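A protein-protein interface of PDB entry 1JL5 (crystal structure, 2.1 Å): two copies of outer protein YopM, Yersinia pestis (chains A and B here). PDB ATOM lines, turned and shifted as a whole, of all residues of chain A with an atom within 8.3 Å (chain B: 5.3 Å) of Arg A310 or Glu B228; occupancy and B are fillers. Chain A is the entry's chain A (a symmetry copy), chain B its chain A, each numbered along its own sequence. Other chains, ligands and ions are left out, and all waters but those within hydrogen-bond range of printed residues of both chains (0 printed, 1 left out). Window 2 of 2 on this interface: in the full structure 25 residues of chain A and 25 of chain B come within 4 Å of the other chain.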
ATOM      1  N   PHE A 289      31.936  32.710  18.545  1.00  0.00           N
ATOM      2  CA  PHE A 289      31.668  31.604  17.654  1.00  0.00           C
ATOM      3  C   PHE A 289      30.732  30.654  18.363  1.00  0.00           C
ATOM      4  O   PHE A 289      30.962  30.291  19.515  1.00  0.00           O
ATOM      5  CB  PHE A 289      32.966  30.882  17.316  1.00  0.00           C
ATOM      6  CG  PHE A 289      33.849  31.656  16.406  1.00  0.00           C
ATOM      7  CD1 PHE A 289      33.615  31.662  15.038  1.00  0.00           C
ATOM      8  CD2 PHE A 289      34.897  32.413  16.914  1.00  0.00           C
ATOM      9  CE1 PHE A 289      34.410  32.420  14.189  1.00  0.00           C
ATOM     10  CE2 PHE A 289      35.693  33.171  16.075  1.00  0.00           C
ATOM     11  CZ  PHE A 289      35.450  33.173  14.708  1.00  0.00           C
ATOM     12  N   SER A 290      29.661  30.274  17.686  1.00  0.00           N
ATOM     13  CA  SER A 290      28.712  29.333  18.260  1.00  0.00           C
ATOM     14  C   SER A 290      29.177  27.969  17.773  1.00  0.00           C
ATOM     15  O   SER A 290      28.677  26.926  18.185  1.00  0.00           O
ATOM     16  CB  SER A 290      27.299  29.639  17.772  1.00  0.00           C
ATOM     17  OG  SER A 290      27.278  29.747  16.366  1.00  0.00           O
ATOM     18  N   GLY A 291      30.165  28.001  16.893  1.00  0.00           N
ATOM     19  CA  GLY A 291      30.727  26.780  16.365  1.00  0.00           C
ATOM     20  C   GLY A 291      31.817  27.111  15.370  1.00  0.00           C
ATOM     21  O   GLY A 291      32.060  28.271  15.057  1.00  0.00           O
ATOM     22  N   LEU A 292      32.493  26.080  14.894  1.00  0.00           N
ATOM     23  CA  LEU A 292      33.529  26.240  13.898  1.00  0.00           C
ATOM     24  C   LEU A 292      33.116  25.260  12.822  1.00  0.00           C
ATOM     25  O   LEU A 292      33.190  24.049  13.006  1.00  0.00           O
ATOM     26  CB  LEU A 292      34.900  25.889  14.475  1.00  0.00           C
ATOM     27  CG  LEU A 292      35.376  26.893  15.529  1.00  0.00           C
ATOM     28  CD1 LEU A 292      36.724  26.461  16.085  1.00  0.00           C
ATOM     29  CD2 LEU A 292      35.470  28.285  14.898  1.00  0.00           C
ATOM     30  N   ASN A 307      34.431  30.633  23.585  1.00  0.00           N
ATOM     31  CA  ASN A 307      33.577  31.113  22.529  1.00  0.00           C
ATOM     32  C   ASN A 307      32.275  30.533  22.998  1.00  0.00           C
ATOM     33  O   ASN A 307      32.089  30.333  24.190  1.00  0.00           O
ATOM     34  CB  ASN A 307      34.000  30.532  21.185  1.00  0.00           C
ATOM     35  CG  ASN A 307      35.015  31.402  20.495  1.00  0.00           C
ATOM     36  OD1 ASN A 307      34.677  32.472  20.001  1.00  0.00           O
ATOM     37  ND2 ASN A 307      36.273  30.970  20.483  1.00  0.00           N
ATOM     38  N   GLU A 308      31.367  30.263  22.086  1.00  0.00           N
ATOM     39  CA  GLU A 308      30.116  29.666  22.490  1.00  0.00           C
ATOM     40  C   GLU A 308      29.987  28.468  21.573  1.00  0.00           C
ATOM     41  O   GLU A 308      28.906  28.125  21.114  1.00  0.00           O
ATOM     42  CB  GLU A 308      28.966  30.651  22.290  1.00  0.00           C
ATOM     43  CG  GLU A 308      27.717  30.233  23.022  1.00  0.00           C
ATOM     44  CD  GLU A 308      27.863  30.342  24.524  1.00  0.00           C
ATOM     45  OE1 GLU A 308      29.009  30.390  25.028  1.00  0.00           O
ATOM     46  OE2 GLU A 308      26.823  30.377  25.205  1.00  0.00           O
ATOM     47  N   ILE A 309      31.129  27.844  21.309  1.00  0.00           N
ATOM     48  CA  ILE A 309      31.184  26.697  20.421  1.00  0.00           C
ATOM     49  C   ILE A 309      30.327  25.565  20.936  1.00  0.00           C
ATOM     50  O   ILE A 309      30.599  24.989  21.987  1.00  0.00           O
ATOM     51  CB  ILE A 309      32.613  26.164  20.261  1.00  0.00           C
ATOM     52  CG1 ILE A 309      33.544  27.280  19.765  1.00  0.00           C
ATOM     53  CG2 ILE A 309      32.612  24.989  19.297  1.00  0.00           C
ATOM     54  CD1 ILE A 309      33.094  27.909  18.500  1.00  0.00           C
ATOM     55  N   ARG A 310      29.289  25.246  20.184  1.00  0.00           N
ATOM     56  CA  ARG A 310      28.401  24.165  20.560  1.00  0.00           C
ATOM     57  C   ARG A 310      28.843  22.915  19.846  1.00  0.00           C
ATOM     58  O   ARG A 310      28.516  21.806  20.254  1.00  0.00           O
ATOM     59  CB  ARG A 310      26.980  24.464  20.133  1.00  0.00           C
ATOM     60  CG  ARG A 310      26.355  25.654  20.779  1.00  0.00           C
ATOM     61  CD  ARG A 310      24.902  25.335  20.883  1.00  0.00           C
ATOM     62  NE  ARG A 310      24.049  26.491  20.724  1.00  0.00           N
ATOM     63  CZ  ARG A 310      22.731  26.405  20.727  1.00  0.00           C
ATOM     64  NH1 ARG A 310      22.162  25.217  20.879  1.00  0.00           N
ATOM     65  NH2 ARG A 310      21.990  27.491  20.588  1.00  0.00           N
ATOM     66  N   SER A 311      29.563  23.101  18.752  1.00  0.00           N
ATOM     67  CA  SER A 311      30.032  21.970  17.990  1.00  0.00           C
ATOM     68  C   SER A 311      31.258  22.360  17.207  1.00  0.00           C
ATOM     69  O   SER A 311      31.416  23.504  16.783  1.00  0.00           O
ATOM     70  CB  SER A 311      28.948  21.486  17.027  1.00  0.00           C
ATOM     71  OG  SER A 311      28.698  22.469  16.042  1.00  0.00           O
ATOM     72  N   LEU A 312      32.134  21.388  17.035  1.00  0.00           N
ATOM     73  CA  LEU A 312      33.350  21.588  16.290  1.00  0.00           C
ATOM     74  C   LEU A 312      33.225  20.767  15.033  1.00  0.00           C
ATOM     75  O   LEU A 312      32.753  19.630  15.068  1.00  0.00           O
ATOM     76  CB  LEU A 312      34.557  21.083  17.073  1.00  0.00           C
ATOM     77  CG  LEU A 312      35.089  21.916  18.225  1.00  0.00           C
ATOM     78  CD1 LEU A 312      36.306  21.216  18.816  1.00  0.00           C
ATOM     79  CD2 LEU A 312      35.463  23.302  17.713  1.00  0.00           C
ATOM     80  N   CYS A 313      33.636  21.351  13.920  1.00  0.00           N
ATOM     81  CA  CYS A 313      33.619  20.640  12.660  1.00  0.00           C
ATOM     82  C   CYS A 313      34.712  19.601  12.846  1.00  0.00           C
ATOM     83  O   CYS A 313      35.404  19.598  13.866  1.00  0.00           O
ATOM     84  CB  CYS A 313      34.013  21.585  11.541  1.00  0.00           C
ATOM     85  SG  CYS A 313      35.554  22.432  11.933  1.00  0.00           S
ATOM     86  N   ASN A 327      33.701  26.278  26.306  1.00  0.00           N
ATOM     87  CA  ASN A 327      32.784  26.460  25.211  1.00  0.00           C
ATOM     88  C   ASN A 327      31.532  25.753  25.627  1.00  0.00           C
ATOM     89  O   ASN A 327      31.312  25.553  26.815  1.00  0.00           O
ATOM     90  CB  ASN A 327      33.363  25.908  23.919  1.00  0.00           C
ATOM     91  CG  ASN A 327      34.205  26.938  23.204  1.00  0.00           C
ATOM     92  OD1 ASN A 327      33.689  27.965  22.763  1.00  0.00           O
ATOM     93  ND2 ASN A 327      35.502  26.687  23.105  1.00  0.00           N
ATOM     94  N   LYS A 328      30.695  25.386  24.675  1.00  0.00           N
ATOM     95  CA  LYS A 328      29.460  24.722  25.030  1.00  0.00           C
ATOM     96  C   LYS A 328      29.376  23.409  24.299  1.00  0.00           C
ATOM     97  O   LYS A 328      28.313  22.980  23.867  1.00  0.00           O
ATOM     98  CB  LYS A 328      28.278  25.623  24.695  1.00  0.00           C
ATOM     99  CG  LYS A 328      28.342  26.955  25.431  1.00  0.00           C
ATOM    100  CD  LYS A 328      28.243  26.743  26.931  1.00  0.00           C
ATOM    101  CE  LYS A 328      28.587  28.009  27.701  1.00  0.00           C
ATOM    102  NZ  LYS A 328      27.739  29.171  27.312  1.00  0.00           N
ATOM    103  N   LEU A 329      30.532  22.774  24.189  1.00  0.00           N
ATOM    104  CA  LEU A 329      30.645  21.498  23.521  1.00  0.00           C
ATOM    105  C   LEU A 329      30.132  20.389  24.411  1.00  0.00           C
ATOM    106  O   LEU A 329      30.547  20.256  25.561  1.00  0.00           O
ATOM    107  CB  LEU A 329      32.104  21.220  23.171  1.00  0.00           C
ATOM    108  CG  LEU A 329      32.672  22.151  22.106  1.00  0.00           C
ATOM    109  CD1 LEU A 329      34.187  22.050  22.078  1.00  0.00           C
ATOM    110  CD2 LEU A 329      32.066  21.787  20.764  1.00  0.00           C
ATOM    111  N   ILE A 330      29.208  19.604  23.886  1.00  0.00           N
ATOM    112  CA  ILE A 330      28.708  18.479  24.645  1.00  0.00           C
ATOM    113  C   ILE A 330      29.428  17.276  24.049  1.00  0.00           C
ATOM    114  O   ILE A 330      29.376  16.168  24.571  1.00  0.00           O
ATOM    115  CB  ILE A 330      27.183  18.332  24.500  1.00  0.00           C
ATOM    116  CG1 ILE A 330      26.810  18.200  23.027  1.00  0.00           C
ATOM    117  CG2 ILE A 330      26.485  19.523  25.125  1.00  0.00           C
ATOM    118  CD1 ILE A 330      26.374  16.819  22.637  1.00  0.00           C
ATOM    119  N   GLU A 331      30.137  17.526  22.958  1.00  0.00           N
ATOM    120  CA  GLU A 331      30.869  16.476  22.294  1.00  0.00           C
ATOM    121  C   GLU A 331      31.989  17.037  21.438  1.00  0.00           C
ATOM    122  O   GLU A 331      31.839  18.073  20.793  1.00  0.00           O
ATOM    123  CB  GLU A 331      29.912  15.654  21.432  1.00  0.00           C
ATOM    124  CG  GLU A 331      30.501  14.388  20.864  1.00  0.00           C
ATOM    125  CD  GLU A 331      29.429  13.513  20.241  1.00  0.00           C
ATOM    126  OE1 GLU A 331      28.805  13.957  19.256  1.00  0.00           O
ATOM    127  OE2 GLU A 331      29.214  12.385  20.737  1.00  0.00           O
ATOM    128  N   LEU A 332      33.127  16.357  21.459  1.00  0.00           N
ATOM    129  CA  LEU A 332      34.255  16.765  20.650  1.00  0.00           C
ATOM    130  C   LEU A 332      34.251  15.870  19.434  1.00  0.00           C
ATOM    131  O   LEU A 332      33.819  14.723  19.501  1.00  0.00           O
ATOM    132  CB  LEU A 332      35.565  16.569  21.403  1.00  0.00           C
ATOM    133  CG  LEU A 332      35.824  17.494  22.587  1.00  0.00           C
ATOM    134  CD1 LEU A 332      37.111  17.081  23.270  1.00  0.00           C
ATOM    135  CD2 LEU A 332      35.903  18.934  22.102  1.00  0.00           C
ATOM    136  N   PRO A 333      34.706  16.387  18.291  1.00  0.00           N
ATOM    137  CA  PRO A 333      34.718  15.523  17.114  1.00  0.00           C
ATOM    138  C   PRO A 333      35.858  14.529  17.297  1.00  0.00           C
ATOM    139  O   PRO A 333      36.615  14.621  18.270  1.00  0.00           O
ATOM    140  CB  PRO A 333      34.983  16.498  15.973  1.00  0.00           C
ATOM    141  CG  PRO A 333      35.842  17.529  16.624  1.00  0.00           C
ATOM    142  CD  PRO A 333      35.162  17.743  17.955  1.00  0.00           C
ATOM    143  N   ASN A 347      33.589  22.582  29.374  1.00  0.00           N
ATOM    144  CA  ASN A 347      32.671  22.344  28.289  1.00  0.00           C
ATOM    145  C   ASN A 347      31.629  21.432  28.863  1.00  0.00           C
ATOM    146  O   ASN A 347      31.626  21.182  30.061  1.00  0.00           O
ATOM    147  CB  ASN A 347      33.385  21.698  27.113  1.00  0.00           C
ATOM    148  CG  ASN A 347      33.988  22.721  26.197  1.00  0.00           C
ATOM    149  OD1 ASN A 347      33.270  23.422  25.489  1.00  0.00           O
ATOM    150  ND2 ASN A 347      35.306  22.836  26.219  1.00  0.00           N
ATOM    151  N   HIS A 348      30.744  20.940  28.015  1.00  0.00           N
ATOM    152  CA  HIS A 348      29.697  20.064  28.480  1.00  0.00           C
ATOM    153  C   HIS A 348      29.917  18.670  27.926  1.00  0.00           C
ATOM    154  O   HIS A 348      28.983  18.014  27.475  1.00  0.00           O
ATOM    155  CB  HIS A 348      28.347  20.583  28.027  1.00  0.00           C
ATOM    156  CG  HIS A 348      27.253  20.276  28.990  1.00  0.00           C
ATOM    157  ND1 HIS A 348      26.973  21.086  30.067  1.00  0.00           N
ATOM    158  CD2 HIS A 348      26.423  19.214  29.087  1.00  0.00           C
ATOM    159  CE1 HIS A 348      26.015  20.536  30.787  1.00  0.00           C
ATOM    160  NE2 HIS A 348      25.664  19.399  30.215  1.00  0.00           N
ATOM    161  N   LEU A 349      31.163  18.226  27.960  1.00  0.00           N
ATOM    162  CA  LEU A 349      31.502  16.911  27.447  1.00  0.00           C
ATOM    163  C   LEU A 349      31.107  15.806  28.408  1.00  0.00           C
ATOM    164  O   LEU A 349      31.463  15.834  29.581  1.00  0.00           O
ATOM    165  CB  LEU A 349      33.001  16.824  27.179  1.00  0.00           C
ATOM    166  CG  LEU A 349      33.547  17.888  26.234  1.00  0.00           C
ATOM    167  CD1 LEU A 349      35.033  17.660  26.047  1.00  0.00           C
ATOM    168  CD2 LEU A 349      32.799  17.841  24.901  1.00  0.00           C
ATOM    169  N   LYS B 208      18.096  20.951  28.398  1.00  0.00           N
ATOM    170  CA  LYS B 208      18.040  21.782  27.211  1.00  0.00           C
ATOM    171  C   LYS B 208      16.994  22.832  27.525  1.00  0.00           C
ATOM    172  O   LYS B 208      17.043  23.955  27.023  1.00  0.00           O
ATOM    173  CB  LYS B 208      17.626  20.976  25.986  1.00  0.00           C
ATOM    174  CG  LYS B 208      18.686  20.007  25.510  1.00  0.00           C
ATOM    175  CD  LYS B 208      18.325  19.464  24.145  1.00  0.00           C
ATOM    176  CE  LYS B 208      19.389  18.521  23.622  1.00  0.00           C
ATOM    177  NZ  LYS B 208      19.066  18.055  22.242  1.00  0.00           N
ATOM    178  N   LYS B 209      16.051  22.451  28.376  1.00  0.00           N
ATOM    179  CA  LYS B 209      14.993  23.352  28.788  1.00  0.00           C
ATOM    180  C   LYS B 209      14.676  23.108  30.242  1.00  0.00           C
ATOM    181  O   LYS B 209      14.972  22.056  30.789  1.00  0.00           O
ATOM    182  CB  LYS B 209      13.729  23.110  27.953  1.00  0.00           C
ATOM    183  CG  LYS B 209      13.910  23.393  26.471  1.00  0.00           C
ATOM    184  CD  LYS B 209      12.599  23.269  25.699  1.00  0.00           C
ATOM    185  CE  LYS B 209      12.809  23.591  24.222  1.00  0.00           C
ATOM    186  NZ  LYS B 209      11.544  23.523  23.439  1.00  0.00           N
ATOM    187  N   ILE B 226      22.384  22.892  29.124  1.00  0.00           N
ATOM    188  CA  ILE B 226      22.454  23.238  27.722  1.00  0.00           C
ATOM    189  C   ILE B 226      21.126  23.881  27.405  1.00  0.00           C
ATOM    190  O   ILE B 226      20.472  23.568  26.418  1.00  0.00           O
ATOM    191  CB  ILE B 226      22.732  21.999  26.853  1.00  0.00           C
ATOM    192  CG1 ILE B 226      21.841  20.834  27.281  1.00  0.00           C
ATOM    193  CG2 ILE B 226      24.200  21.614  26.988  1.00  0.00           C
ATOM    194  CD1 ILE B 226      22.169  19.533  26.565  1.00  0.00           C
ATOM    195  N   LEU B 227      20.734  24.783  28.298  1.00  0.00           N
ATOM    196  CA  LEU B 227      19.490  25.513  28.162  1.00  0.00           C
ATOM    197  C   LEU B 227      19.574  26.455  26.984  1.00  0.00           C
ATOM    198  O   LEU B 227      20.414  27.357  26.954  1.00  0.00           O
ATOM    199  CB  LEU B 227      19.203  26.300  29.437  1.00  0.00           C
ATOM    200  CG  LEU B 227      18.999  25.426  30.672  1.00  0.00           C
ATOM    201  CD1 LEU B 227      18.783  26.303  31.894  1.00  0.00           C
ATOM    202  CD2 LEU B 227      17.810  24.505  30.441  1.00  0.00           C
ATOM    203  N   GLU B 228      18.700  26.220  26.011  1.00  0.00           N
ATOM    204  CA  GLU B 228      18.623  27.032  24.805  1.00  0.00           C
ATOM    205  C   GLU B 228      17.938  28.315  25.210  1.00  0.00           C
ATOM    206  O   GLU B 228      18.155  29.369  24.631  1.00  0.00           O
ATOM    207  CB  GLU B 228      17.759  26.340  23.754  1.00  0.00           C
ATOM    208  CG  GLU B 228      18.193  24.940  23.363  1.00  0.00           C
ATOM    209  CD  GLU B 228      19.475  24.931  22.563  1.00  0.00           C
ATOM    210  OE1 GLU B 228      19.627  25.808  21.688  1.00  0.00           O
ATOM    211  OE2 GLU B 228      20.315  24.043  22.802  1.00  0.00           O
ATOM    212  N   GLU B 229      17.090  28.200  26.218  1.00  0.00           N
ATOM    213  CA  GLU B 229      16.339  29.333  26.712  1.00  0.00           C
ATOM    214  C   GLU B 229      15.867  29.019  28.108  1.00  0.00           C
ATOM    215  O   GLU B 229      15.890  27.872  28.545  1.00  0.00           O
ATOM    216  CB  GLU B 229      15.124  29.586  25.825  1.00  0.00           C
ATOM    217  CG  GLU B 229      14.239  28.365  25.695  1.00  0.00           C
ATOM    218  CD  GLU B 229      13.003  28.607  24.857  1.00  0.00           C
ATOM    219  OE1 GLU B 229      13.125  29.219  23.773  1.00  0.00           O
ATOM    220  OE2 GLU B 229      11.911  28.171  25.284  1.00  0.00           O
ATOM    221  N   LEU B 230      15.442  30.058  28.808  1.00  0.00           N
ATOM    222  CA  LEU B 230      14.925  29.906  30.148  1.00  0.00           C
ATOM    223  C   LEU B 230      13.418  29.885  29.989  1.00  0.00           C
ATOM    224  O   LEU B 230      12.886  30.430  29.030  1.00  0.00           O
ATOM    225  CB  LEU B 230      15.348  31.094  31.010  1.00  0.00           C
ATOM    226  CG  LEU B 230      16.842  31.168  31.320  1.00  0.00           C
ATOM    227  CD1 LEU B 230      17.128  32.369  32.214  1.00  0.00           C
ATOM    228  CD2 LEU B 230      17.270  29.878  32.005  1.00  0.00           C
ATOM    229  N   LEU B 248      23.091  27.863  26.891  1.00  0.00           N
ATOM    230  CA  LEU B 248      23.084  28.249  25.497  1.00  0.00           C
ATOM    231  C   LEU B 248      22.064  29.345  25.305  1.00  0.00           C
ATOM    232  O   LEU B 248      21.355  29.383  24.305  1.00  0.00           O
ATOM    233  CB  LEU B 248      22.741  27.038  24.641  1.00  0.00           C
ATOM    234  CG  LEU B 248      23.772  25.924  24.798  1.00  0.00           C
ATOM    235  CD1 LEU B 248      23.276  24.655  24.123  1.00  0.00           C
ATOM    236  CD2 LEU B 248      25.086  26.387  24.198  1.00  0.00           C
ATOM    237  N   LEU B 249      21.999  30.244  26.275  1.00  0.00           N
ATOM    238  CA  LEU B 249      21.055  31.343  26.216  1.00  0.00           C
ATOM    239  C   LEU B 249      21.508  32.420  25.252  1.00  0.00           C
ATOM    240  O   LEU B 249      22.660  32.845  25.287  1.00  0.00           O
ATOM    241  CB  LEU B 249      20.875  31.943  27.604  1.00  0.00           C
ATOM    242  CG  LEU B 249      20.411  30.971  28.687  1.00  0.00           C
ATOM    243  CD1 LEU B 249      20.257  31.724  30.008  1.00  0.00           C
ATOM    244  CD2 LEU B 249      19.095  30.319  28.268  1.00  0.00           C
ATOM    245  N   LYS B 250      20.597  32.850  24.386  1.00  0.00           N
ATOM    246  CA  LYS B 250      20.883  33.907  23.419  1.00  0.00           C
ATOM    247  C   LYS B 250      20.143  35.135  23.926  1.00  0.00           C
ATOM    248  O   LYS B 250      20.477  36.271  23.601  1.00  0.00           O
ATOM    249  CB  LYS B 250      20.352  33.548  22.029  1.00  0.00           C
ATOM    250  CG  LYS B 250      20.777  32.196  21.499  1.00  0.00           C
ATOM    251  CD  LYS B 250      19.998  31.083  22.182  1.00  0.00           C
ATOM    252  CE  LYS B 250      20.367  29.719  21.630  1.00  0.00           C
ATOM    253  NZ  LYS B 250      19.680  28.640  22.389  1.00  0.00           N
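Printed residues of chain B that touch a printed residue of chain A: Ile B226, Glu B228, Leu B248 and Lys B250.
Hydrophobic or aromatic side chains of chain B that line the printed part of chain A: Ile B226 and Leu B248.
Among the printed residues, 6 pairs touch across the chains.
The backbone carbonyl oxygen of Leu B248 is in hydrogen-bond range of the side-chain amino group of Lys B250, at 2.7 Å.
O of Leu B227 sits at hydrogen-bond distance from N of Leu B248 (2.7 Å).
The backbone NH of Arg A310 is in hydrogen-bond range of the backbone carbonyl oxygen of Ser A290 (2.7 Å).
The side-chain amino group of Lys B250 lies within salt-bridge range of the side-chain carboxylate of Glu B228, at 2.9 Å.
The side-chain amino group (NZ) of Lys A328 is in salt-bridge range of the side-chain carboxylate (OE2) of Glu A308.
The backbone NH of Lys A328 sits at hydrogen-bond distance from the side-chain amide oxygen of Asn A347 (3.3 Å).
No position is printed for both chains.
Of the 6 pairs that touch across the chains among the printed residues, none has its exchanged pair printed and touching as well.
Leu B248 touches Arg A310.
Lys A328 touches Leu B248.
Ile A330 touches Ile B226.
His A348 touches Ile B226 (CD2 to CG2, 3.9 Å).
The guanidinium group (NH2) of Arg A310 lies close to the side-chain amino group (NZ) of Lys B250, 3.1 Å away.
The side-chain carboxylate of Glu B228 lies within salt-bridge range of the guanidinium group of Arg A310 (2.7 Å).
Arg A310 touches just these residues of chain B: Glu B228, Leu B248 and Lys B250.
Ser A311 touches none of the printed residues of chain B.
Asn A327 touches none of the printed residues of chain B.
Printed residues of chain B within 4 Å of Lys A328: Leu B248 (3.3 Å).
Printed residues of chain A within 4 Å of Ile B226: Ile A330 (3.6 Å) and His A348 (3.9 Å).
Of chain A, only Arg A310 comes within 4 Å of Glu B228.
Printed residues of chain A within 4 Å of Lys B250: Arg A310 (2.9 Å).
The nearest printed residue of chain B that does not touch Arg A310 is Ile B226 (6.0 Å).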
